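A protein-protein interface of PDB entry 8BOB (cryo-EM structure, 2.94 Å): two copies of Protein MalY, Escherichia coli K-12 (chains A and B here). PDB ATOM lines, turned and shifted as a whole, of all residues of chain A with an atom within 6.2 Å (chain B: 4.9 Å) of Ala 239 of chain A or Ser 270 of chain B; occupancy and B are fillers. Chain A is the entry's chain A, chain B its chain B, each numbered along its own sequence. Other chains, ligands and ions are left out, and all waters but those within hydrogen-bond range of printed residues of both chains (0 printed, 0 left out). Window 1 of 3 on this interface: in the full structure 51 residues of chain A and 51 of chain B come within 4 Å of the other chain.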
ATOM      1  N   ASN A 236     -13.967  -8.673  27.579  1.00  0.00           N
ATOM      2  CA  ASN A 236     -14.805  -9.209  26.511  1.00  0.00           C
ATOM      3  C   ASN A 236     -16.103  -8.413  26.392  1.00  0.00           C
ATOM      4  O   ASN A 236     -17.201  -8.930  26.576  1.00  0.00           O
ATOM      5  CB  ASN A 236     -15.081 -10.695  26.739  1.00  0.00           C
ATOM      6  CG  ASN A 236     -15.899 -11.308  25.641  1.00  0.00           C
ATOM      7  OD1 ASN A 236     -15.512 -11.290  24.479  1.00  0.00           O
ATOM      8  ND2 ASN A 236     -17.044 -11.861  26.005  1.00  0.00           N
ATOM      9  N   ILE A 237     -15.953  -7.125  26.111  1.00  0.00           N
ATOM     10  CA  ILE A 237     -17.104  -6.263  25.865  1.00  0.00           C
ATOM     11  C   ILE A 237     -16.864  -5.343  24.675  1.00  0.00           C
ATOM     12  O   ILE A 237     -17.154  -4.146  24.776  1.00  0.00           O
ATOM     13  CB  ILE A 237     -17.435  -5.423  27.106  1.00  0.00           C
ATOM     14  CG1 ILE A 237     -16.178  -4.730  27.621  1.00  0.00           C
ATOM     15  CG2 ILE A 237     -18.037  -6.278  28.184  1.00  0.00           C
ATOM     16  CD1 ILE A 237     -16.434  -3.706  28.679  1.00  0.00           C
ATOM     17  N   PRO A 238     -16.373  -5.822  23.528  1.00  0.00           N
ATOM     18  CA  PRO A 238     -16.198  -4.910  22.395  1.00  0.00           C
ATOM     19  C   PRO A 238     -17.500  -4.453  21.780  1.00  0.00           C
ATOM     20  O   PRO A 238     -17.488  -3.511  20.983  1.00  0.00           O
ATOM     21  CB  PRO A 238     -15.383  -5.740  21.407  1.00  0.00           C
ATOM     22  CG  PRO A 238     -15.751  -7.099  21.705  1.00  0.00           C
ATOM     23  CD  PRO A 238     -15.966  -7.187  23.169  1.00  0.00           C
ATOM     24  N   ALA A 239     -18.619  -5.079  22.122  1.00  0.00           N
ATOM     25  CA  ALA A 239     -19.922  -4.695  21.604  1.00  0.00           C
ATOM     26  C   ALA A 239     -20.499  -3.489  22.305  1.00  0.00           C
ATOM     27  O   ALA A 239     -21.674  -3.182  22.114  1.00  0.00           O
ATOM     28  CB  ALA A 239     -20.897  -5.860  21.721  1.00  0.00           C
ATOM     29  N   LEU A 240     -19.707  -2.820  23.126  1.00  0.00           N
ATOM     30  CA  LEU A 240     -20.077  -1.628  23.872  1.00  0.00           C
ATOM     31  C   LEU A 240     -19.079  -0.532  23.585  1.00  0.00           C
ATOM     32  O   LEU A 240     -18.469   0.038  24.487  1.00  0.00           O
ATOM     33  CB  LEU A 240     -20.153  -1.905  25.366  1.00  0.00           C
ATOM     34  CG  LEU A 240     -21.462  -2.433  25.924  1.00  0.00           C
ATOM     35  CD1 LEU A 240     -21.719  -3.792  25.414  1.00  0.00           C
ATOM     36  CD2 LEU A 240     -21.369  -2.486  27.414  1.00  0.00           C
ATOM     37  N   THR A 241     -18.881  -0.256  22.300  1.00  0.00           N
ATOM     38  CA  THR A 241     -17.766   0.531  21.791  1.00  0.00           C
ATOM     39  C   THR A 241     -17.338   1.653  22.722  1.00  0.00           C
ATOM     40  O   THR A 241     -18.162   2.467  23.137  1.00  0.00           O
ATOM     41  CB  THR A 241     -18.146   1.136  20.444  1.00  0.00           C
ATOM     42  OG1 THR A 241     -19.328   1.926  20.607  1.00  0.00           O
ATOM     43  CG2 THR A 241     -18.426   0.049  19.443  1.00  0.00           C
ATOM     44  N   SER A 270     -20.997   6.552  24.804  1.00  0.00           N
ATOM     45  CA  SER A 270     -21.996   5.532  25.068  1.00  0.00           C
ATOM     46  C   SER A 270     -22.082   5.351  26.573  1.00  0.00           C
ATOM     47  O   SER A 270     -21.191   4.753  27.177  1.00  0.00           O
ATOM     48  CB  SER A 270     -21.624   4.227  24.378  1.00  0.00           C
ATOM     49  OG  SER A 270     -22.314   3.149  24.973  1.00  0.00           O
ATOM     50  N   PHE B  59     -21.000 -10.141  24.983  1.00  0.00           N
ATOM     51  CA  PHE B  59     -20.958  -8.906  24.215  1.00  0.00           C
ATOM     52  C   PHE B  59     -19.788  -8.921  23.259  1.00  0.00           C
ATOM     53  O   PHE B  59     -19.028  -7.963  23.159  1.00  0.00           O
ATOM     54  CB  PHE B  59     -20.866  -7.691  25.118  1.00  0.00           C
ATOM     55  CG  PHE B  59     -22.042  -7.518  26.014  1.00  0.00           C
ATOM     56  CD1 PHE B  59     -23.158  -6.845  25.585  1.00  0.00           C
ATOM     57  CD2 PHE B  59     -22.034  -8.028  27.287  1.00  0.00           C
ATOM     58  CE1 PHE B  59     -24.234  -6.682  26.407  1.00  0.00           C
ATOM     59  CE2 PHE B  59     -23.110  -7.868  28.107  1.00  0.00           C
ATOM     60  CZ  PHE B  59     -24.211  -7.198  27.667  1.00  0.00           C
ATOM     61  N   GLY B  60     -19.622 -10.020  22.542  1.00  0.00           N
ATOM     62  CA  GLY B  60     -18.568 -10.114  21.562  1.00  0.00           C
ATOM     63  C   GLY B  60     -18.878  -9.275  20.341  1.00  0.00           C
ATOM     64  O   GLY B  60     -19.842  -8.513  20.289  1.00  0.00           O
ATOM     65  N   SER B  62     -20.124  -7.957  16.856  1.00  0.00           N
ATOM     66  CA  SER B  62     -21.416  -8.086  16.214  1.00  0.00           C
ATOM     67  C   SER B  62     -21.336  -7.456  14.838  1.00  0.00           C
ATOM     68  O   SER B  62     -20.377  -6.760  14.509  1.00  0.00           O
ATOM     69  CB  SER B  62     -22.513  -7.430  17.045  1.00  0.00           C
ATOM     70  OG  SER B  62     -22.880  -8.274  18.115  1.00  0.00           O
ATOM     71  N   TYR B  92     -24.268   2.116   8.043  1.00  0.00           N
ATOM     72  CA  TYR B  92     -24.246   2.429   9.461  1.00  0.00           C
ATOM     73  C   TYR B  92     -23.181   3.475   9.748  1.00  0.00           C
ATOM     74  O   TYR B  92     -22.225   3.645   8.992  1.00  0.00           O
ATOM     75  CB  TYR B  92     -23.988   1.162  10.275  1.00  0.00           C
ATOM     76  CG  TYR B  92     -23.765   1.376  11.744  1.00  0.00           C
ATOM     77  CD1 TYR B  92     -24.824   1.390  12.627  1.00  0.00           C
ATOM     78  CD2 TYR B  92     -22.490   1.542  12.251  1.00  0.00           C
ATOM     79  CE1 TYR B  92     -24.621   1.578  13.968  1.00  0.00           C
ATOM     80  CE2 TYR B  92     -22.281   1.736  13.583  1.00  0.00           C
ATOM     81  CZ  TYR B  92     -23.347   1.752  14.439  1.00  0.00           C
ATOM     82  OH  TYR B  92     -23.134   1.943  15.778  1.00  0.00           O
ATOM     83  N   THR B 241     -25.208   5.573  21.115  1.00  0.00           N
ATOM     84  CA  THR B 241     -24.746   6.120  19.847  1.00  0.00           C
ATOM     85  C   THR B 241     -24.953   5.184  18.669  1.00  0.00           C
ATOM     86  O   THR B 241     -24.532   4.029  18.710  1.00  0.00           O
ATOM     87  CB  THR B 241     -23.261   6.451  19.949  1.00  0.00           C
ATOM     88  OG1 THR B 241     -22.546   5.267  20.312  1.00  0.00           O
ATOM     89  CG2 THR B 241     -23.030   7.499  21.004  1.00  0.00           C
ATOM     90  N   SER B 268     -17.254  -1.675  14.001  1.00  0.00           N
ATOM     91  CA  SER B 268     -17.922  -2.501  14.987  1.00  0.00           C
ATOM     92  C   SER B 268     -19.058  -1.706  15.608  1.00  0.00           C
ATOM     93  O   SER B 268     -18.796  -0.685  16.254  1.00  0.00           O
ATOM     94  CB  SER B 268     -16.940  -2.958  16.052  1.00  0.00           C
ATOM     95  OG  SER B 268     -17.600  -3.696  17.056  1.00  0.00           O
ATOM     96  N   PRO B 269     -20.308  -2.103  15.433  1.00  0.00           N
ATOM     97  CA  PRO B 269     -21.418  -1.306  15.947  1.00  0.00           C
ATOM     98  C   PRO B 269     -21.627  -1.547  17.430  1.00  0.00           C
ATOM     99  O   PRO B 269     -21.005  -2.405  18.047  1.00  0.00           O
ATOM    100  CB  PRO B 269     -22.601  -1.833  15.148  1.00  0.00           C
ATOM    101  CG  PRO B 269     -22.287  -3.246  15.002  1.00  0.00           C
ATOM    102  CD  PRO B 269     -20.797  -3.320  14.778  1.00  0.00           C
ATOM    103  N   SER B 270     -22.535  -0.768  17.993  1.00  0.00           N
ATOM    104  CA  SER B 270     -22.984  -0.972  19.359  1.00  0.00           C
ATOM    105  C   SER B 270     -24.194  -1.888  19.314  1.00  0.00           C
ATOM    106  O   SER B 270     -25.283  -1.459  18.932  1.00  0.00           O
ATOM    107  CB  SER B 270     -23.327   0.357  20.014  1.00  0.00           C
ATOM    108  OG  SER B 270     -24.159   0.148  21.133  1.00  0.00           O
ATOM    109  N   VAL B 271     -24.006  -3.151  19.695  1.00  0.00           N
ATOM    110  CA  VAL B 271     -25.084  -4.129  19.590  1.00  0.00           C
ATOM    111  C   VAL B 271     -26.342  -3.642  20.288  1.00  0.00           C
ATOM    112  O   VAL B 271     -27.461  -3.948  19.858  1.00  0.00           O
ATOM    113  CB  VAL B 271     -24.621  -5.494  20.141  1.00  0.00           C
ATOM    114  CG1 VAL B 271     -24.428  -5.437  21.629  1.00  0.00           C
ATOM    115  CG2 VAL B 271     -25.623  -6.562  19.801  1.00  0.00           C
ATOM    116  N   LEU B 272     -26.196  -2.853  21.347  1.00  0.00           N
ATOM    117  CA  LEU B 272     -27.379  -2.375  22.043  1.00  0.00           C
ATOM    118  C   LEU B 272     -28.078  -1.266  21.277  1.00  0.00           C
ATOM    119  O   LEU B 272     -29.300  -1.147  21.356  1.00  0.00           O
ATOM    120  CB  LEU B 272     -27.014  -1.916  23.448  1.00  0.00           C
ATOM    121  CG  LEU B 272     -26.560  -3.067  24.340  1.00  0.00           C
ATOM    122  CD1 LEU B 272     -26.435  -2.624  25.764  1.00  0.00           C
ATOM    123  CD2 LEU B 272     -27.532  -4.200  24.243  1.00  0.00           C
ATOM    124  N   ALA B 273     -27.341  -0.472  20.503  1.00  0.00           N
ATOM    125  CA  ALA B 273     -27.996   0.493  19.632  1.00  0.00           C
ATOM    126  C   ALA B 273     -28.835  -0.205  18.577  1.00  0.00           C
ATOM    127  O   ALA B 273     -29.957   0.217  18.286  1.00  0.00           O
ATOM    128  CB  ALA B 273     -26.965   1.399  18.972  1.00  0.00           C
ATOM    129  N   LEU B 274     -28.310  -1.278  17.990  1.00  0.00           N
ATOM    130  CA  LEU B 274     -29.087  -2.022  17.010  1.00  0.00           C
ATOM    131  C   LEU B 274     -30.305  -2.665  17.650  1.00  0.00           C
ATOM    132  O   LEU B 274     -31.393  -2.655  17.068  1.00  0.00           O
ATOM    133  CB  LEU B 274     -28.220  -3.079  16.339  1.00  0.00           C
ATOM    134  CG  LEU B 274     -26.887  -2.616  15.772  1.00  0.00           C
ATOM    135  CD1 LEU B 274     -26.147  -3.794  15.217  1.00  0.00           C
ATOM    136  CD2 LEU B 274     -27.097  -1.583  14.709  1.00  0.00           C
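O of Phe 59 of chain B lies within hydrogen-bond range of N of Ala 239 of chain A, at 3.1 Å.
N of Val 271 of chain B lies within hydrogen-bond range of O of Ala 239 of chain A (3.4 Å).
O of Phe 59 of chain B lies close to N of Pro 238 of chain A.
OG of Ser 270 of chain B is in hydrogen-bond range of N of Ala 273 of chain B, at 3.3 Å.
Asn 236 of chain A touches Phe 59 of chain B (O to O, 3.99 Å).
O of Phe 59 of chain B touches C of Ile 237 of chain A, 3.7 Å away.
Pro 238 of chain A touches Ser 268 of chain B.
Ala 239 of chain A touches Gly 60 of chain B (CB to O, 3.2 Å).
Ser 270 of chain B touches Ala 239 of chain A.
Leu 240 of chain A touches Phe 59 of chain B.
Thr 241 of chain A touches Ser 268 of chain B.
O of Pro 269 of chain B touches CG2 of Thr 241 of chain A (3.8 Å).
Of the printed residues of chain B, Ala 239 of chain A touches Phe 59, Gly 60, Ser 270 and Val 271.
Of the printed residues of chain A, Phe 59 of chain B touches Asn 236 (3.99 Å), Ile 237 (3.7 Å), Pro 238 (3.2 Å), Ala 239 (3.1 Å) and Leu 240 (3.4 Å).
Printed residues of chain A within 4 Å of Pro 269 of chain B: Thr 241.
Of chain A, only Ala 239 (3.8 Å) comes within 4 Å of Ser 270 of chain B.
Of the printed residues of chain A, Val 271 of chain B touches Ala 239 (3.4 Å).
Leu 272 of chain B touches none of the printed residues of chain A.
The nearest residue of chain B that does not touch Ala 239 of chain A is Pro 269 of chain B (4.2 Å).
The nearest residue of chain A that does not touch Ser 270 of chain B is Thr 241 of chain A (4.3 Å).
The nearest printed residue of chain A that does not touch Pro 269 of chain B is Ala 239 of chain A (4.2 Å).
Hydrophobic or aromatic side chains of chain A that line the printed part of chain B: Pro 238, Ala 239 and Leu 240.
Hydrophobic or aromatic side chains of chain B that line the printed part of chain A: Phe 59 and Val 271.
Positions printed for both chains: 241 and 270.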
